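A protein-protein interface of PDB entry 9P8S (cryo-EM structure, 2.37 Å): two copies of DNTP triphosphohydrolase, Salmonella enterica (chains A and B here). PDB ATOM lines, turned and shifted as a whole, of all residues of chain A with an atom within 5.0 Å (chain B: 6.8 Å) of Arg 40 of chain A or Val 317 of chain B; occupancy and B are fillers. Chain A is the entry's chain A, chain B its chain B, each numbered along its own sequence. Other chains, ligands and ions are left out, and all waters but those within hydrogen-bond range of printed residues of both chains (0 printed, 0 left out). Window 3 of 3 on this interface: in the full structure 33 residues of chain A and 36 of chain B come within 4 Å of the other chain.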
ATOM      1  N   ARG A  31      15.288 -28.204  24.667  1.00  0.00           N
ATOM      2  CA  ARG A  31      14.064 -28.154  25.456  1.00  0.00           C
ATOM      3  C   ARG A  31      13.767 -29.501  26.099  1.00  0.00           C
ATOM      4  O   ARG A  31      14.094 -30.550  25.544  1.00  0.00           O
ATOM      5  CB  ARG A  31      12.876 -27.731  24.589  1.00  0.00           C
ATOM      6  CG  ARG A  31      13.079 -26.444  23.813  1.00  0.00           C
ATOM      7  CD  ARG A  31      11.830 -26.095  23.022  1.00  0.00           C
ATOM      8  NE  ARG A  31      11.402 -27.199  22.170  1.00  0.00           N
ATOM      9  CZ  ARG A  31      10.305 -27.190  21.427  1.00  0.00           C
ATOM     10  NH1 ARG A  31       9.492 -26.147  21.405  1.00  0.00           N
ATOM     11  NH2 ARG A  31      10.013 -28.257  20.687  1.00  0.00           N
ATOM     12  N   ARG A  36       8.170 -29.155  25.435  1.00  0.00           N
ATOM     13  CA  ARG A  36       7.727 -29.425  24.075  1.00  0.00           C
ATOM     14  C   ARG A  36       6.245 -29.776  24.044  1.00  0.00           C
ATOM     15  O   ARG A  36       5.537 -29.410  23.101  1.00  0.00           O
ATOM     16  CB  ARG A  36       8.569 -30.545  23.464  1.00  0.00           C
ATOM     17  CG  ARG A  36       8.173 -30.936  22.050  1.00  0.00           C
ATOM     18  CD  ARG A  36       8.109 -32.446  21.904  1.00  0.00           C
ATOM     19  NE  ARG A  36       7.373 -32.866  20.717  1.00  0.00           N
ATOM     20  CZ  ARG A  36       6.170 -33.424  20.742  1.00  0.00           C
ATOM     21  NH1 ARG A  36       5.525 -33.627  21.880  1.00  0.00           N
ATOM     22  NH2 ARG A  36       5.600 -33.787  19.598  1.00  0.00           N
ATOM     23  N   ASP A  37       5.756 -30.484  25.065  1.00  0.00           N
ATOM     24  CA  ASP A  37       4.328 -30.780  25.143  1.00  0.00           C
ATOM     25  C   ASP A  37       3.509 -29.500  25.227  1.00  0.00           C
ATOM     26  O   ASP A  37       2.490 -29.350  24.541  1.00  0.00           O
ATOM     27  CB  ASP A  37       4.033 -31.671  26.349  1.00  0.00           C
ATOM     28  CG  ASP A  37       4.269 -33.132  26.064  1.00  0.00           C
ATOM     29  OD1 ASP A  37       4.817 -33.444  24.988  1.00  0.00           O
ATOM     30  OD2 ASP A  37       3.895 -33.967  26.910  1.00  0.00           O
ATOM     31  N   TYR A  38       3.939 -28.566  26.076  1.00  0.00           N
ATOM     32  CA  TYR A  38       3.227 -27.296  26.180  1.00  0.00           C
ATOM     33  C   TYR A  38       3.256 -26.544  24.858  1.00  0.00           C
ATOM     34  O   TYR A  38       2.250 -25.952  24.447  1.00  0.00           O
ATOM     35  CB  TYR A  38       3.816 -26.432  27.294  1.00  0.00           C
ATOM     36  CG  TYR A  38       3.203 -25.050  27.349  1.00  0.00           C
ATOM     37  CD1 TYR A  38       1.982 -24.836  27.970  1.00  0.00           C
ATOM     38  CD2 TYR A  38       3.844 -23.960  26.776  1.00  0.00           C
ATOM     39  CE1 TYR A  38       1.416 -23.578  28.018  1.00  0.00           C
ATOM     40  CE2 TYR A  38       3.286 -22.700  26.820  1.00  0.00           C
ATOM     41  CZ  TYR A  38       2.072 -22.514  27.442  1.00  0.00           C
ATOM     42  OH  TYR A  38       1.513 -21.259  27.490  1.00  0.00           O
ATOM     43  N   ASP A  39       4.405 -26.550  24.178  1.00  0.00           N
ATOM     44  CA  ASP A  39       4.498 -25.873  22.888  1.00  0.00           C
ATOM     45  C   ASP A  39       3.561 -26.500  21.860  1.00  0.00           C
ATOM     46  O   ASP A  39       2.877 -25.786  21.117  1.00  0.00           O
ATOM     47  CB  ASP A  39       5.940 -25.896  22.387  1.00  0.00           C
ATOM     48  CG  ASP A  39       6.904 -25.255  23.363  1.00  0.00           C
ATOM     49  OD1 ASP A  39       6.443 -24.741  24.404  1.00  0.00           O
ATOM     50  OD2 ASP A  39       8.123 -25.267  23.094  1.00  0.00           O
ATOM     51  N   ARG A  40       3.512 -27.832  21.808  1.00  0.00           N
ATOM     52  CA  ARG A  40       2.624 -28.503  20.864  1.00  0.00           C
ATOM     53  C   ARG A  40       1.166 -28.200  21.173  1.00  0.00           C
ATOM     54  O   ARG A  40       0.355 -28.016  20.260  1.00  0.00           O
ATOM     55  CB  ARG A  40       2.863 -30.014  20.880  1.00  0.00           C
ATOM     56  CG  ARG A  40       4.280 -30.439  20.547  1.00  0.00           C
ATOM     57  CD  ARG A  40       4.736 -29.927  19.193  1.00  0.00           C
ATOM     58  NE  ARG A  40       6.189 -29.952  19.082  1.00  0.00           N
ATOM     59  CZ  ARG A  40       6.870 -30.795  18.320  1.00  0.00           C
ATOM     60  NH1 ARG A  40       6.257 -31.701  17.575  1.00  0.00           N
ATOM     61  NH2 ARG A  40       8.198 -30.729  18.304  1.00  0.00           N
ATOM     62  N   ILE A  41       0.810 -28.157  22.459  1.00  0.00           N
ATOM     63  CA  ILE A  41      -0.559 -27.816  22.833  1.00  0.00           C
ATOM     64  C   ILE A  41      -0.892 -26.397  22.393  1.00  0.00           C
ATOM     65  O   ILE A  41      -1.978 -26.134  21.863  1.00  0.00           O
ATOM     66  CB  ILE A  41      -0.765 -28.003  24.347  1.00  0.00           C
ATOM     67  CG1 ILE A  41      -0.730 -29.486  24.710  1.00  0.00           C
ATOM     68  CG2 ILE A  41      -2.082 -27.390  24.786  1.00  0.00           C
ATOM     69  CD1 ILE A  41      -0.845 -29.749  26.190  1.00  0.00           C
ATOM     70  N   LEU A  42       0.037 -25.462  22.601  1.00  0.00           N
ATOM     71  CA  LEU A  42      -0.218 -24.077  22.222  1.00  0.00           C
ATOM     72  C   LEU A  42      -0.364 -23.929  20.713  1.00  0.00           C
ATOM     73  O   LEU A  42      -1.219 -23.172  20.236  1.00  0.00           O
ATOM     74  CB  LEU A  42       0.897 -23.172  22.742  1.00  0.00           C
ATOM     75  CG  LEU A  42       0.755 -21.696  22.367  1.00  0.00           C
ATOM     76  CD1 LEU A  42      -0.588 -21.154  22.824  1.00  0.00           C
ATOM     77  CD2 LEU A  42       1.884 -20.885  22.961  1.00  0.00           C
ATOM     78  N   PHE A  43       0.455 -24.642  19.944  1.00  0.00           N
ATOM     79  CA  PHE A  43       0.415 -24.521  18.492  1.00  0.00           C
ATOM     80  C   PHE A  43      -0.678 -25.364  17.848  1.00  0.00           C
ATOM     81  O   PHE A  43      -0.837 -25.306  16.625  1.00  0.00           O
ATOM     82  CB  PHE A  43       1.771 -24.900  17.893  1.00  0.00           C
ATOM     83  CG  PHE A  43       2.782 -23.791  17.933  1.00  0.00           C
ATOM     84  CD1 PHE A  43       3.612 -23.632  19.026  1.00  0.00           C
ATOM     85  CD2 PHE A  43       2.901 -22.909  16.876  1.00  0.00           C
ATOM     86  CE1 PHE A  43       4.542 -22.614  19.065  1.00  0.00           C
ATOM     87  CE2 PHE A  43       3.830 -21.890  16.910  1.00  0.00           C
ATOM     88  CZ  PHE A  43       4.651 -21.743  18.007  1.00  0.00           C
ATOM     89  N   ALA A  44      -1.426 -26.139  18.627  1.00  0.00           N
ATOM     90  CA  ALA A  44      -2.466 -26.988  18.066  1.00  0.00           C
ATOM     91  C   ALA A  44      -3.622 -26.155  17.526  1.00  0.00           C
ATOM     92  O   ALA A  44      -3.934 -25.075  18.035  1.00  0.00           O
ATOM     93  CB  ALA A  44      -2.979 -27.970  19.118  1.00  0.00           C
ATOM     94  N   LEU A 182      -1.120 -35.640  19.447  1.00  0.00           N
ATOM     95  CA  LEU A 182      -0.015 -34.722  19.696  1.00  0.00           C
ATOM     96  C   LEU A 182       1.195 -35.399  20.326  1.00  0.00           C
ATOM     97  O   LEU A 182       2.241 -34.753  20.455  1.00  0.00           O
ATOM     98  CB  LEU A 182      -0.473 -33.569  20.594  1.00  0.00           C
ATOM     99  CG  LEU A 182      -1.815 -32.902  20.292  1.00  0.00           C
ATOM    100  CD1 LEU A 182      -1.995 -31.673  21.166  1.00  0.00           C
ATOM    101  CD2 LEU A 182      -1.926 -32.533  18.822  1.00  0.00           C
ATOM    102  N   ASN B  77       5.736 -17.530  23.781  1.00  0.00           N
ATOM    103  CA  ASN B  77       6.230 -18.886  23.997  1.00  0.00           C
ATOM    104  C   ASN B  77       7.631 -19.063  23.425  1.00  0.00           C
ATOM    105  O   ASN B  77       8.497 -19.677  24.061  1.00  0.00           O
ATOM    106  CB  ASN B  77       5.271 -19.899  23.378  1.00  0.00           C
ATOM    107  CG  ASN B  77       5.737 -21.326  23.562  1.00  0.00           C
ATOM    108  OD1 ASN B  77       5.980 -22.040  22.590  1.00  0.00           O
ATOM    109  ND2 ASN B  77       5.865 -21.749  24.812  1.00  0.00           N
ATOM    110  N   VAL B 250       7.304 -18.035   9.696  1.00  0.00           N
ATOM    111  CA  VAL B 250       6.915 -19.443   9.706  1.00  0.00           C
ATOM    112  C   VAL B 250       5.402 -19.587   9.823  1.00  0.00           C
ATOM    113  O   VAL B 250       4.774 -20.352   9.081  1.00  0.00           O
ATOM    114  CB  VAL B 250       7.643 -20.193  10.834  1.00  0.00           C
ATOM    115  CG1 VAL B 250       7.258 -21.659  10.821  1.00  0.00           C
ATOM    116  CG2 VAL B 250       9.143 -20.038  10.684  1.00  0.00           C
ATOM    117  N   MET B 312       2.893 -29.357   6.586  1.00  0.00           N
ATOM    118  CA  MET B 312       3.173 -27.997   7.021  1.00  0.00           C
ATOM    119  C   MET B 312       3.420 -27.926   8.520  1.00  0.00           C
ATOM    120  O   MET B 312       4.242 -27.126   8.967  1.00  0.00           O
ATOM    121  CB  MET B 312       2.025 -27.072   6.627  1.00  0.00           C
ATOM    122  CG  MET B 312       2.398 -25.607   6.662  1.00  0.00           C
ATOM    123  SD  MET B 312       3.942 -25.299   5.787  1.00  0.00           S
ATOM    124  CE  MET B 312       4.498 -23.813   6.611  1.00  0.00           C
ATOM    125  N   GLN B 313       2.730 -28.748   9.309  1.00  0.00           N
ATOM    126  CA  GLN B 313       2.993 -28.784  10.743  1.00  0.00           C
ATOM    127  C   GLN B 313       4.403 -29.282  11.026  1.00  0.00           C
ATOM    128  O   GLN B 313       5.125 -28.707  11.855  1.00  0.00           O
ATOM    129  CB  GLN B 313       1.955 -29.666  11.437  1.00  0.00           C
ATOM    130  CG  GLN B 313       2.376 -30.160  12.804  1.00  0.00           C
ATOM    131  CD  GLN B 313       1.292 -30.967  13.483  1.00  0.00           C
ATOM    132  OE1 GLN B 313       0.165 -31.045  12.997  1.00  0.00           O
ATOM    133  NE2 GLN B 313       1.628 -31.578  14.613  1.00  0.00           N
ATOM    134  N   MET B 314       4.821 -30.348  10.340  1.00  0.00           N
ATOM    135  CA  MET B 314       6.182 -30.838  10.537  1.00  0.00           C
ATOM    136  C   MET B 314       7.212 -29.815  10.073  1.00  0.00           C
ATOM    137  O   MET B 314       8.252 -29.629  10.722  1.00  0.00           O
ATOM    138  CB  MET B 314       6.377 -32.168   9.817  1.00  0.00           C
ATOM    139  CG  MET B 314       7.049 -33.216  10.681  1.00  0.00           C
ATOM    140  SD  MET B 314       6.248 -33.429  12.280  1.00  0.00           S
ATOM    141  CE  MET B 314       7.616 -34.043  13.258  1.00  0.00           C
ATOM    142  N   PHE B 315       6.940 -29.138   8.954  1.00  0.00           N
ATOM    143  CA  PHE B 315       7.838 -28.087   8.493  1.00  0.00           C
ATOM    144  C   PHE B 315       7.918 -26.958   9.506  1.00  0.00           C
ATOM    145  O   PHE B 315       8.996 -26.404   9.740  1.00  0.00           O
ATOM    146  CB  PHE B 315       7.383 -27.547   7.138  1.00  0.00           C
ATOM    147  CG  PHE B 315       8.138 -26.325   6.691  1.00  0.00           C
ATOM    148  CD1 PHE B 315       9.311 -26.446   5.972  1.00  0.00           C
ATOM    149  CD2 PHE B 315       7.676 -25.056   6.993  1.00  0.00           C
ATOM    150  CE1 PHE B 315      10.007 -25.329   5.564  1.00  0.00           C
ATOM    151  CE2 PHE B 315       8.370 -23.938   6.590  1.00  0.00           C
ATOM    152  CZ  PHE B 315       9.536 -24.074   5.874  1.00  0.00           C
ATOM    153  N   ARG B 316       6.783 -26.581  10.095  1.00  0.00           N
ATOM    154  CA  ARG B 316       6.786 -25.538  11.109  1.00  0.00           C
ATOM    155  C   ARG B 316       7.646 -25.941  12.293  1.00  0.00           C
ATOM    156  O   ARG B 316       8.454 -25.145  12.780  1.00  0.00           O
ATOM    157  CB  ARG B 316       5.360 -25.243  11.569  1.00  0.00           C
ATOM    158  CG  ARG B 316       5.269 -24.148  12.614  1.00  0.00           C
ATOM    159  CD  ARG B 316       4.010 -24.272  13.451  1.00  0.00           C
ATOM    160  NE  ARG B 316       4.079 -25.391  14.383  1.00  0.00           N
ATOM    161  CZ  ARG B 316       3.126 -26.300  14.529  1.00  0.00           C
ATOM    162  NH1 ARG B 316       2.015 -26.258  13.815  1.00  0.00           N
ATOM    163  NH2 ARG B 316       3.293 -27.278  15.416  1.00  0.00           N
ATOM    164  N   VAL B 317       7.502 -27.185  12.754  1.00  0.00           N
ATOM    165  CA  VAL B 317       8.308 -27.650  13.880  1.00  0.00           C
ATOM    166  C   VAL B 317       9.792 -27.564  13.544  1.00  0.00           C
ATOM    167  O   VAL B 317      10.586 -26.979  14.295  1.00  0.00           O
ATOM    168  CB  VAL B 317       7.900 -29.081  14.274  1.00  0.00           C
ATOM    169  CG1 VAL B 317       8.975 -29.720  15.135  1.00  0.00           C
ATOM    170  CG2 VAL B 317       6.569 -29.069  15.003  1.00  0.00           C
ATOM    171  N   TYR B 318      10.182 -28.120  12.394  1.00  0.00           N
ATOM    172  CA  TYR B 318      11.597 -28.154  12.031  1.00  0.00           C
ATOM    173  C   TYR B 318      12.158 -26.748  11.847  1.00  0.00           C
ATOM    174  O   TYR B 318      13.236 -26.423  12.361  1.00  0.00           O
ATOM    175  CB  TYR B 318      11.791 -28.978  10.760  1.00  0.00           C
ATOM    176  CG  TYR B 318      11.782 -30.468  10.992  1.00  0.00           C
ATOM    177  CD1 TYR B 318      12.433 -31.022  12.084  1.00  0.00           C
ATOM    178  CD2 TYR B 318      11.121 -31.321  10.121  1.00  0.00           C
ATOM    179  CE1 TYR B 318      12.427 -32.384  12.301  1.00  0.00           C
ATOM    180  CE2 TYR B 318      11.110 -32.684  10.330  1.00  0.00           C
ATOM    181  CZ  TYR B 318      11.764 -33.211  11.422  1.00  0.00           C
ATOM    182  OH  TYR B 318      11.755 -34.569  11.636  1.00  0.00           O
ATOM    183  N   ALA B 319      11.437 -25.898  11.113  1.00  0.00           N
ATOM    184  CA  ALA B 319      11.924 -24.556  10.824  1.00  0.00           C
ATOM    185  C   ALA B 319      12.004 -23.710  12.085  1.00  0.00           C
ATOM    186  O   ALA B 319      12.971 -22.967  12.272  1.00  0.00           O
ATOM    187  CB  ALA B 319      11.028 -23.887   9.785  1.00  0.00           C
ATOM    188  N   ILE B 320      10.998 -23.800  12.957  1.00  0.00           N
ATOM    189  CA  ILE B 320      11.031 -23.038  14.199  1.00  0.00           C
ATOM    190  C   ILE B 320      12.195 -23.495  15.064  1.00  0.00           C
ATOM    191  O   ILE B 320      12.916 -22.671  15.636  1.00  0.00           O
ATOM    192  CB  ILE B 320       9.687 -23.157  14.937  1.00  0.00           C
ATOM    193  CG1 ILE B 320       8.663 -22.202  14.322  1.00  0.00           C
ATOM    194  CG2 ILE B 320       9.858 -22.863  16.418  1.00  0.00           C
ATOM    195  CD1 ILE B 320       7.384 -22.084  15.112  1.00  0.00           C
ATOM    196  N   ALA B 321      12.413 -24.810  15.160  1.00  0.00           N
ATOM    197  CA  ALA B 321      13.537 -25.305  15.949  1.00  0.00           C
ATOM    198  C   ALA B 321      14.862 -24.792  15.399  1.00  0.00           C
ATOM    199  O   ALA B 321      15.708 -24.292  16.152  1.00  0.00           O
ATOM    200  CB  ALA B 321      13.520 -26.832  15.983  1.00  0.00           C
ATOM    201  N   GLU B 322      15.051 -24.887  14.080  1.00  0.00           N
ATOM    202  CA  GLU B 322      16.311 -24.454  13.483  1.00  0.00           C
ATOM    203  C   GLU B 322      16.529 -22.957  13.658  1.00  0.00           C
ATOM    204  O   GLU B 322      17.629 -22.520  14.020  1.00  0.00           O
ATOM    205  CB  GLU B 322      16.343 -24.828  12.002  1.00  0.00           C
ATOM    206  CG  GLU B 322      16.466 -26.317  11.743  1.00  0.00           C
ATOM    207  CD  GLU B 322      17.906 -26.784  11.702  1.00  0.00           C
ATOM    208  OE1 GLU B 322      18.810 -25.945  11.893  1.00  0.00           O
ATOM    209  OE2 GLU B 322      18.135 -27.991  11.479  1.00  0.00           O
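The side-chain carboxylate of Asp 39 of chain A sits at hydrogen-bond distance from the side-chain amide nitrogen of Asn 77 of chain B, 3.1 Å away.
OD2 of Asp 39 of chain A is in salt-bridge range of NE of Arg 31 of chain A (3.9 Å).
Asn 77 of chain B touches Tyr 38 of chain A. CG1 of Val 317 of chain B touches NH2 of Arg 40 of chain A, at 3.4 Å. Leu 42 of chain A touches Asn 77 of chain B. CE1 of Phe 43 of chain A touches OD1 of Asn 77 of chain B (3.9 Å). CD2 of Phe 43 of chain A touches NE of Arg 316 of chain B, at 3.7 Å. CE2 of Phe 43 of chain A touches CD1 of Ile 320 of chain B, at 3.99 Å.
Of chain B, only Val 317 (3.4 Å) comes within 4 Å of Arg 40 of chain A. Val 317 of chain B touches just one residue of chain A: Arg 40. Of the printed residues of chain B, Tyr 38 of chain A touches Asn 77. Of the printed residues of chain B, Leu 42 of chain A touches Asn 77 (3.6 Å). Printed residues of chain A within 4 Å of Arg 316 of chain B: Phe 43. Of the printed residues of chain B, Phe 43 of chain A touches Asn 77 (3.9 Å), Arg 316 (3.7 Å) and Ile 320 (3.99 Å). Met 314 of chain B touches none of the printed residues of chain A. The nearest residue of chain B that does not touch Arg 40 of chain A is Arg 316 of chain B (4.8 Å). The nearest printed residue of chain A that does not touch Arg 316 of chain B is Arg 40 of chain A (4.8 Å).
Of the 13 printed residues of chain B, 4 touch a printed residue of chain A. Printed residues of chain B that touch a printed residue of chain A: Asn 77, Arg 316, Val 317 and Ile 320. Hydrophobic or aromatic side chains of chain B within 4 Å of the printed part of chain A: Val 317 and Ile 320. Hydrophobic or aromatic side chains of chain A within 4 Å of the printed part of chain B: Tyr 38, Leu 42 and Phe 43. Among the printed residues, 7 pairs touch across the chains. Among the printed residues, no Asp or Glu carboxylate lies within 4 Å of a Lys or Arg side-chain nitrogen of the other chain.
No position is printed for both chains. Of the 7 pairs that touch across the chains among the printed residues, none has its exchanged pair printed and touching as well.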
